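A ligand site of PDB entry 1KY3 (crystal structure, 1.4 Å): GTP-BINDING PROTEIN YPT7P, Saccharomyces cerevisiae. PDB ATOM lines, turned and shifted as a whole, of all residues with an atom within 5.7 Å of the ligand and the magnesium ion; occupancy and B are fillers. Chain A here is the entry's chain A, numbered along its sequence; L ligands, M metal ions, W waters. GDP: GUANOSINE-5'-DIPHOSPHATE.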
ATOM      1  N   GLY A  15     -16.506   0.753   2.073  1.00  0.00           N
ATOM      2  CA  GLY A  15     -17.918   0.635   1.745  1.00  0.00           C
ATOM      3  C   GLY A  15     -18.515   1.980   1.376  1.00  0.00           C
ATOM      4  O   GLY A  15     -17.932   3.036   1.653  1.00  0.00           O
ATOM      5  N   ASP A  16     -19.685   1.922   0.750  1.00  0.00           N
ATOM      6  CA  ASP A  16     -20.359   3.122   0.276  1.00  0.00           C
ATOM      7  C   ASP A  16     -20.587   4.102   1.425  1.00  0.00           C
ATOM      8  O   ASP A  16     -20.757   3.786   2.632  1.00  0.00           O
ATOM      9  CB  ASP A  16     -21.682   2.764  -0.391  1.00  0.00           C
ATOM     10  CG  ASP A  16     -21.580   2.102  -1.753  1.00  0.00           C
ATOM     11  OD1 ASP A  16     -20.462   1.873  -2.247  1.00  0.00           O
ATOM     12  OD2 ASP A  16     -22.645   1.787  -2.357  1.00  0.00           O
ATOM     13  N   SER A  17     -20.566   5.394   1.064  1.00  0.00           N
ATOM     14  CA  SER A  17     -20.948   6.385   2.056  1.00  0.00           C
ATOM     15  C   SER A  17     -22.326   6.088   2.647  1.00  0.00           C
ATOM     16  O   SER A  17     -23.268   5.745   1.927  1.00  0.00           O
ATOM     17  CB  SER A  17     -20.941   7.762   1.352  1.00  0.00           C
ATOM     18  OG  SER A  17     -21.202   8.755   2.304  1.00  0.00           O
ATOM     19  N   GLY A  18     -22.511   6.226   3.967  1.00  0.00           N
ATOM     20  CA  GLY A  18     -23.848   6.052   4.548  1.00  0.00           C
ATOM     21  C   GLY A  18     -24.081   4.724   5.181  1.00  0.00           C
ATOM     22  O   GLY A  18     -25.093   4.570   5.864  1.00  0.00           O
ATOM     23  N   VAL A  19     -23.225   3.750   5.020  1.00  0.00           N
ATOM     24  CA  VAL A  19     -23.556   2.402   5.530  1.00  0.00           C
ATOM     25  C   VAL A  19     -23.320   2.210   7.007  1.00  0.00           C
ATOM     26  O   VAL A  19     -23.902   1.239   7.596  1.00  0.00           O
ATOM     27  CB  VAL A  19     -22.777   1.320   4.756  1.00  0.00           C
ATOM     28  CG1 VAL A  19     -23.148   1.398   3.277  1.00  0.00           C
ATOM     29  CG2 VAL A  19     -21.276   1.467   4.907  1.00  0.00           C
ATOM     30  N   GLY A  20     -22.536   3.083   7.600  1.00  0.00           N
ATOM     31  CA  GLY A  20     -22.251   3.042   9.043  1.00  0.00           C
ATOM     32  C   GLY A  20     -20.808   2.714   9.358  1.00  0.00           C
ATOM     33  O   GLY A  20     -20.563   2.240  10.468  1.00  0.00           O
ATOM     34  N   LYS A  21     -19.821   2.934   8.470  1.00  0.00           N
ATOM     35  CA  LYS A  21     -18.430   2.605   8.747  1.00  0.00           C
ATOM     36  C   LYS A  21     -17.948   3.356   9.982  1.00  0.00           C
ATOM     37  O   LYS A  21     -17.373   2.780  10.897  1.00  0.00           O
ATOM     38  CB  LYS A  21     -17.544   2.984   7.533  1.00  0.00           C
ATOM     39  CG  LYS A  21     -17.921   2.155   6.288  1.00  0.00           C
ATOM     40  CD  LYS A  21     -17.097   2.480   5.076  1.00  0.00           C
ATOM     41  CE  LYS A  21     -17.057   3.958   4.720  1.00  0.00           C
ATOM     42  NZ  LYS A  21     -18.411   4.443   4.290  1.00  0.00           N
ATOM     43  N   THR A  22     -18.129   4.684   9.995  1.00  0.00           N
ATOM     44  CA  THR A  22     -17.678   5.490  11.135  1.00  0.00           C
ATOM     45  C   THR A  22     -18.350   5.066  12.449  1.00  0.00           C
ATOM     46  O   THR A  22     -17.772   4.960  13.525  1.00  0.00           O
ATOM     47  CB  THR A  22     -17.909   6.991  10.816  1.00  0.00           C
ATOM     48  OG1 THR A  22     -17.143   7.311   9.653  1.00  0.00           O
ATOM     49  CG2 THR A  22     -17.424   7.860  11.975  1.00  0.00           C
ATOM     50  N   SER A  23     -19.635   4.781  12.357  1.00  0.00           N
ATOM     51  CA  SER A  23     -20.402   4.362  13.532  1.00  0.00           C
ATOM     52  C   SER A  23     -19.924   3.001  14.054  1.00  0.00           C
ATOM     53  O   SER A  23     -19.855   2.770  15.265  1.00  0.00           O
ATOM     54  CB  SER A  23     -21.912   4.267  13.182  1.00  0.00           C
ATOM     55  OG  SER A  23     -22.435   5.534  12.822  1.00  0.00           O
ATOM     56  N   LEU A  24     -19.568   2.085  13.145  1.00  0.00           N
ATOM     57  CA  LEU A  24     -19.038   0.797  13.573  1.00  0.00           C
ATOM     58  C   LEU A  24     -17.707   0.958  14.291  1.00  0.00           C
ATOM     59  O   LEU A  24     -17.480   0.333  15.315  1.00  0.00           O
ATOM     60  CB  LEU A  24     -18.878  -0.147  12.373  1.00  0.00           C
ATOM     61  CG  LEU A  24     -20.220  -0.730  11.900  1.00  0.00           C
ATOM     62  CD1 LEU A  24     -20.090  -1.192  10.458  1.00  0.00           C
ATOM     63  CD2 LEU A  24     -20.635  -1.869  12.813  1.00  0.00           C
ATOM     64  N   TYR A  33     -22.619   5.181  20.564  1.00  0.00           N
ATOM     65  CA  TYR A  33     -23.295   5.572  19.340  1.00  0.00           C
ATOM     66  C   TYR A  33     -23.996   6.908  19.579  1.00  0.00           C
ATOM     67  O   TYR A  33     -24.738   7.047  20.545  1.00  0.00           O
ATOM     68  CB  TYR A  33     -24.337   4.556  18.870  1.00  0.00           C
ATOM     69  CG  TYR A  33     -25.166   4.997  17.669  1.00  0.00           C
ATOM     70  CD1 TYR A  33     -24.694   4.834  16.376  1.00  0.00           C
ATOM     71  CD2 TYR A  33     -26.415   5.571  17.828  1.00  0.00           C
ATOM     72  CE1 TYR A  33     -25.460   5.239  15.292  1.00  0.00           C
ATOM     73  CE2 TYR A  33     -27.184   5.988  16.779  1.00  0.00           C
ATOM     74  CZ  TYR A  33     -26.691   5.805  15.504  1.00  0.00           C
ATOM     75  OH  TYR A  33     -27.465   6.216  14.439  1.00  0.00           O
ATOM     76  N   SER A  34     -23.763   7.822  18.638  1.00  0.00           N
ATOM     77  CA  SER A  34     -24.638   8.996  18.673  1.00  0.00           C
ATOM     78  C   SER A  34     -25.094   9.275  17.240  1.00  0.00           C
ATOM     79  O   SER A  34     -24.324   9.195  16.278  1.00  0.00           O
ATOM     80  CB  SER A  34     -23.998  10.238  19.283  1.00  0.00           C
ATOM     81  OG  SER A  34     -24.559  11.366  18.633  1.00  0.00           O
ATOM     82  N   GLN A  35     -26.364   9.634  17.146  1.00  0.00           N
ATOM     83  CA  GLN A  35     -26.908  10.063  15.860  1.00  0.00           C
ATOM     84  C   GLN A  35     -26.193  11.351  15.442  1.00  0.00           C
ATOM     85  O   GLN A  35     -26.058  11.665  14.263  1.00  0.00           O
ATOM     86  N   ASP A  64     -10.471   4.499   8.943  1.00  0.00           N
ATOM     87  CA  ASP A  64     -11.772   4.839   8.372  1.00  0.00           C
ATOM     88  C   ASP A  64     -11.435   5.674   7.146  1.00  0.00           C
ATOM     89  O   ASP A  64     -10.373   6.307   6.982  1.00  0.00           O
ATOM     90  CB  ASP A  64     -12.593   5.557   9.423  1.00  0.00           C
ATOM     91  CG  ASP A  64     -14.056   5.730   9.178  1.00  0.00           C
ATOM     92  OD1 ASP A  64     -14.631   6.573   9.890  1.00  0.00           O
ATOM     93  OD2 ASP A  64     -14.707   5.118   8.310  1.00  0.00           O
ATOM     94  N   THR A  65     -12.329   5.702   6.189  1.00  0.00           N
ATOM     95  CA  THR A  65     -12.052   6.340   4.912  1.00  0.00           C
ATOM     96  C   THR A  65     -11.940   7.850   5.104  1.00  0.00           C
ATOM     97  O   THR A  65     -11.327   8.556   4.290  1.00  0.00           O
ATOM     98  CB  THR A  65     -13.217   5.955   4.001  1.00  0.00           C
ATOM     99  OG1 THR A  65     -14.345   6.742   4.440  1.00  0.00           O
ATOM    100  CG2 THR A  65     -13.538   4.466   4.165  1.00  0.00           C
ATOM    101  N   ALA A  66     -12.561   8.276   6.171  1.00  0.00           N
ATOM    102  CA  ALA A  66     -12.737   9.533   6.835  1.00  0.00           C
ATOM    103  C   ALA A  66     -12.716  10.743   5.907  1.00  0.00           C
ATOM    104  O   ALA A  66     -13.562  11.631   6.065  1.00  0.00           O
ATOM    105  CB  ALA A  66     -11.668   9.730   7.931  1.00  0.00           C
ATOM    106  N   ASN A 126     -24.570  -4.018   7.953  1.00  0.00           N
ATOM    107  CA  ASN A 126     -24.954  -3.165   9.086  1.00  0.00           C
ATOM    108  C   ASN A 126     -26.396  -2.691   9.021  1.00  0.00           C
ATOM    109  O   ASN A 126     -27.032  -2.759   7.958  1.00  0.00           O
ATOM    110  CB  ASN A 126     -23.982  -1.965   9.126  1.00  0.00           C
ATOM    111  CG  ASN A 126     -24.035  -1.143  10.388  1.00  0.00           C
ATOM    112  OD1 ASN A 126     -24.038   0.128  10.319  1.00  0.00           O
ATOM    113  ND2 ASN A 126     -24.009  -1.811  11.527  1.00  0.00           N
ATOM    114  N   LYS A 127     -26.876  -2.186  10.132  1.00  0.00           N
ATOM    115  CA  LYS A 127     -28.221  -1.667  10.390  1.00  0.00           C
ATOM    116  C   LYS A 127     -29.242  -2.783  10.516  1.00  0.00           C
ATOM    117  O   LYS A 127     -30.424  -2.608  10.176  1.00  0.00           O
ATOM    118  CB  LYS A 127     -28.679  -0.649   9.311  1.00  0.00           C
ATOM    119  CG  LYS A 127     -27.580   0.426   9.136  1.00  0.00           C
ATOM    120  CD  LYS A 127     -28.125   1.659   8.448  1.00  0.00           C
ATOM    121  CE  LYS A 127     -26.993   2.627   8.050  1.00  0.00           C
ATOM    122  NZ  LYS A 127     -27.550   3.756   7.219  1.00  0.00           N
ATOM    123  N   ILE A 128     -28.829  -3.932  11.073  1.00  0.00           N
ATOM    124  CA  ILE A 128     -29.744  -5.077  11.271  1.00  0.00           C
ATOM    125  C   ILE A 128     -30.786  -4.731  12.311  1.00  0.00           C
ATOM    126  O   ILE A 128     -31.765  -5.529  12.482  1.00  0.00           O
ATOM    127  CB  ILE A 128     -28.948  -6.344  11.656  1.00  0.00           C
ATOM    128  CG1 ILE A 128     -29.651  -7.681  11.428  1.00  0.00           C
ATOM    129  CG2 ILE A 128     -28.454  -6.294  13.100  1.00  0.00           C
ATOM    130  CD1 ILE A 128     -30.178  -7.856   9.997  1.00  0.00           C
ATOM    131  N   ASP A 129     -30.674  -3.611  13.024  1.00  0.00           N
ATOM    132  CA  ASP A 129     -31.722  -3.155  13.947  1.00  0.00           C
ATOM    133  C   ASP A 129     -32.916  -2.584  13.217  1.00  0.00           C
ATOM    134  O   ASP A 129     -33.968  -2.306  13.825  1.00  0.00           O
ATOM    135  CB  ASP A 129     -31.161  -2.030  14.881  1.00  0.00           C
ATOM    136  CG  ASP A 129     -30.665  -0.872  14.002  1.00  0.00           C
ATOM    137  OD1 ASP A 129     -31.415   0.111  13.830  1.00  0.00           O
ATOM    138  OD2 ASP A 129     -29.511  -0.982  13.483  1.00  0.00           O
ATOM    139  N   ALA A 130     -32.824  -2.346  11.931  1.00  0.00           N
ATOM    140  CA  ALA A 130     -33.905  -1.658  11.204  1.00  0.00           C
ATOM    141  C   ALA A 130     -35.165  -2.499  11.187  1.00  0.00           C
ATOM    142  O   ALA A 130     -35.115  -3.728  11.232  1.00  0.00           O
ATOM    143  CB  ALA A 130     -33.451  -1.382   9.768  1.00  0.00           C
ATOM    144  N   THR A 157     -24.754  -6.788  11.562  1.00  0.00           N
ATOM    145  CA  THR A 157     -24.431  -5.966  12.720  1.00  0.00           C
ATOM    146  C   THR A 157     -25.366  -4.773  12.900  1.00  0.00           C
ATOM    147  O   THR A 157     -26.022  -4.338  11.970  1.00  0.00           O
ATOM    148  CB  THR A 157     -22.984  -5.365  12.587  1.00  0.00           C
ATOM    149  OG1 THR A 157     -22.908  -4.533  11.409  1.00  0.00           O
ATOM    150  CG2 THR A 157     -21.899  -6.421  12.468  1.00  0.00           C
ATOM    151  N   SER A 158     -25.373  -4.224  14.126  1.00  0.00           N
ATOM    152  CA  SER A 158     -25.914  -2.907  14.375  1.00  0.00           C
ATOM    153  C   SER A 158     -24.963  -2.109  15.232  1.00  0.00           C
ATOM    154  O   SER A 158     -24.819  -2.407  16.409  1.00  0.00           O
ATOM    155  CB  SER A 158     -27.270  -3.014  15.098  1.00  0.00           C
ATOM    156  OG  SER A 158     -27.735  -1.687  15.411  1.00  0.00           O
ATOM    157  N   ALA A 159     -24.279  -1.101  14.669  1.00  0.00           N
ATOM    158  CA  ALA A 159     -23.509  -0.136  15.458  1.00  0.00           C
ATOM    159  C   ALA A 159     -24.413   0.585  16.444  1.00  0.00           C
ATOM    160  O   ALA A 159     -24.057   0.801  17.624  1.00  0.00           O
ATOM    161  CB  ALA A 159     -22.791   0.834  14.515  1.00  0.00           C
ATOM    162  N   LYS A 160     -25.635   0.934  16.006  1.00  0.00           N
ATOM    163  CA  LYS A 160     -26.562   1.693  16.840  1.00  0.00           C
ATOM    164  C   LYS A 160     -27.001   0.923  18.085  1.00  0.00           C
ATOM    165  O   LYS A 160     -26.987   1.516  19.194  1.00  0.00           O
ATOM    166  CB  LYS A 160     -27.786   2.091  16.035  1.00  0.00           C
ATOM    167  CG  LYS A 160     -28.874   2.778  16.850  1.00  0.00           C
ATOM    168  CD  LYS A 160     -30.085   3.026  15.938  1.00  0.00           C
ATOM    169  CE  LYS A 160     -31.260   3.607  16.697  1.00  0.00           C
ATOM    170  NZ  LYS A 160     -31.548   2.774  17.891  1.00  0.00           N
ATOM    171  N   ASN A 161     -27.370  -0.357  17.938  1.00  0.00           N
ATOM    172  CA  ASN A 161     -27.965  -1.083  19.054  1.00  0.00           C
ATOM    173  C   ASN A 161     -26.973  -2.072  19.670  1.00  0.00           C
ATOM    174  O   ASN A 161     -27.337  -2.906  20.526  1.00  0.00           O
ATOM    175  CB  ASN A 161     -29.254  -1.758  18.577  1.00  0.00           C
ATOM    176  CG  ASN A 161     -30.471  -0.870  18.522  1.00  0.00           C
ATOM    177  OD1 ASN A 161     -31.622  -1.318  18.578  1.00  0.00           O
ATOM    178  ND2 ASN A 161     -30.263   0.445  18.469  1.00  0.00           N
HETATM  179  PB  GDP L   1     -20.353   6.067   6.885  1.00  0.00           P
HETATM  180  O1B GDP L   1     -20.292   4.690   6.296  1.00  0.00           O
HETATM  181  O2B GDP L   1     -20.666   7.160   5.863  1.00  0.00           O
HETATM  182  O3B GDP L   1     -19.192   6.420   7.834  1.00  0.00           O
HETATM  183  O3A GDP L   1     -21.697   6.039   7.861  1.00  0.00           O
HETATM  184  PA  GDP L   1     -21.969   6.733   9.246  1.00  0.00           P
HETATM  185  O1A GDP L   1     -21.716   8.196   9.167  1.00  0.00           O
HETATM  186  O2A GDP L   1     -21.349   5.982  10.398  1.00  0.00           O
HETATM  187  O5' GDP L   1     -23.540   6.497   9.394  1.00  0.00           O
HETATM  188  C5' GDP L   1     -24.445   6.908   8.367  1.00  0.00           C
HETATM  189  C4' GDP L   1     -25.786   7.123   8.995  1.00  0.00           C
HETATM  190  O4' GDP L   1     -26.311   5.800   9.319  1.00  0.00           O
HETATM  191  C3' GDP L   1     -25.751   7.990  10.267  1.00  0.00           C
HETATM  192  O3' GDP L   1     -27.030   8.706  10.257  1.00  0.00           O
HETATM  193  C2' GDP L   1     -25.814   6.909  11.350  1.00  0.00           C
HETATM  194  O2' GDP L   1     -26.271   7.421  12.566  1.00  0.00           O
HETATM  195  C1' GDP L   1     -26.665   5.808  10.673  1.00  0.00           C
HETATM  196  N9  GDP L   1     -26.268   4.405  11.271  1.00  0.00           N
HETATM  197  C8  GDP L   1     -24.999   3.955  11.459  1.00  0.00           C
HETATM  198  N7  GDP L   1     -25.021   2.727  11.994  1.00  0.00           N
HETATM  199  C5  GDP L   1     -26.375   2.405  12.132  1.00  0.00           C
HETATM  200  C6  GDP L   1     -26.968   1.239  12.639  1.00  0.00           C
HETATM  201  O6  GDP L   1     -26.370   0.237  13.061  1.00  0.00           O
HETATM  202  N1  GDP L   1     -28.359   1.294  12.635  1.00  0.00           N
HETATM  203  C2  GDP L   1     -29.059   2.379  12.167  1.00  0.00           C
HETATM  204  N2  GDP L   1     -30.399   2.320  12.199  1.00  0.00           N
HETATM  205  N3  GDP L   1     -28.492   3.490  11.681  1.00  0.00           N
HETATM  206  C4  GDP L   1     -27.156   3.429  11.702  1.00  0.00           C
HETATM  207 MG    MG M   1     -17.785   7.851   7.746  1.00  0.00          MG
HETATM  208  O   HOH W   1     -25.328  10.873   8.488  1.00  0.00           O
HETATM  209  O   HOH W   2     -20.909   9.106  12.173  1.00  0.00           O
HETATM  210  O   HOH W   3     -22.123   9.339   5.874  1.00  0.00           O
HETATM  211  O   HOH W   4     -16.325   6.706   6.907  1.00  0.00           O
HETATM  212  O   HOH W   5     -19.271   9.208   8.559  1.00  0.00           O
HETATM  213  O   HOH W   6     -22.855  10.542   9.951  1.00  0.00           O
HETATM  214  O   HOH W   7     -32.356   4.709  13.190  1.00  0.00           O
HETATM  215  O   HOH W   8     -24.009   8.329  13.972  1.00  0.00           O
HETATM  216  O   HOH W   9     -16.453   9.417   7.740  1.00  0.00           O
HETATM  217  O   HOH W  10     -18.332   8.523   5.767  1.00  0.00           O
HETATM  218  O   HOH W  11     -29.524   5.018   8.827  1.00  0.00           O
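Within 4 Å of the magnesium ion: Thr 22.
The side-chain carboxylate (OD1) of Asp 64 lies close to the side-chain hydroxyl (OG1) of Thr 22, at 2.6 Å. The side-chain amino group (NZ) of Lys 21 is in hydrogen-bond range of the backbone carbonyl oxygen (O) of Asp 16 (2.9 Å). O of Gly 15 lies within hydrogen-bond range of NZ of Lys 21 (3.0 Å). O of Gly 18 is in hydrogen-bond range of NZ of Lys 127, at 2.9 Å. The backbone NH (N) of Ala 159 lies close to the side-chain amide nitrogen (ND2) of Asn 126 (3.2 Å). N of Lys 160 lies close to OG of Ser 158. NZ of Lys 160 sits close to ND2 of Asn 161 (2.7 Å). The side-chain amide nitrogen (ND2) of Asn 126 is in hydrogen-bond range of the side-chain hydroxyl (OG1) of Thr 157.
An oxygen (O2A) of the ligand lies within hydrogen-bond range of the backbone NH of Thr 22, 3.5 Å away. The side-chain hydroxyl of Tyr 33 lies within hydrogen-bond range of an oxygen (O2') of the ligand, at 2.5 Å. The side-chain carboxylate (OD2) of Asp 129 is in hydrogen-bond range of a nitrogen (N1) of the ligand, at 2.7 Å. N of Ser 23 sits at hydrogen-bond distance from O2A of the ligand (2.9 Å). An oxygen (O2A) of the ligand sits at hydrogen-bond distance from the side-chain hydroxyl (OG) of Ser 23, at 2.7 Å. N of Lys 21 lies within hydrogen-bond range of O1B of the ligand, 2.8 Å away. The side-chain amino group (NZ) of Lys 21 lies within salt-bridge range of an oxygen (O1B) of the ligand (2.8 Å). An oxygen (O2B) of the ligand lies within hydrogen-bond range of the backbone NH of Gly 18, at 2.8 Å. An oxygen (O6) of the ligand lies within hydrogen-bond range of the backbone NH of Ala 159, 3.0 Å away. An oxygen (O1B) of the ligand sits at hydrogen-bond distance from the backbone NH of Gly 20. N of Lys 160 sits at hydrogen-bond distance from O6 of the ligand, 3.1 Å away. An oxygen (O4') of the ligand is in hydrogen-bond range of the side-chain amino group of Lys 127 (3.2 Å). The side-chain amide oxygen (OD1) of Asn 126 sits close to a nitrogen (N7) of the ligand (3.2 Å). The side-chain hydroxyl (OG) of Ser 158 lies within hydrogen-bond range of an oxygen (O6) of the ligand, at 3.3 Å. The backbone NH (N) of Val 19 lies within hydrogen-bond range of an oxygen (O1B) of the ligand (3.3 Å).
O of Asp 16 touches O1B of the ligand, at 3.8 Å. Ser 17 touches the ligand. Hydrophobic or aromatic side chains within 4 Å of the ligand: Val 19, Tyr 33 and Ala 159. The nearest printed residue that does not touch the ligand is Gln 35 (4.3 Å).
The magnesium ion is bound by an oxygen (O3B) of the ligand (2.0 Å), water W4 (2.0 Å), water W9 (2.1 Å), the side-chain hydroxyl of Thr 22 (2.1 Å), water W10 (2.2 Å) and water W5 (2.2 Å).
Water W4 bridges OD2 of Asp 64 (2.7 Å) and OG1 of Thr 65 (3.2 Å). Water W8 lies within hydrogen-bond range of O of Ser 34 (2.5 Å), O2' of the ligand (2.8 Å) and OG of Ser 23 (3.4 Å). Water W11 bridges NZ of Lys 127 (2.8 Å) and O4' of the ligand (3.3 Å).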
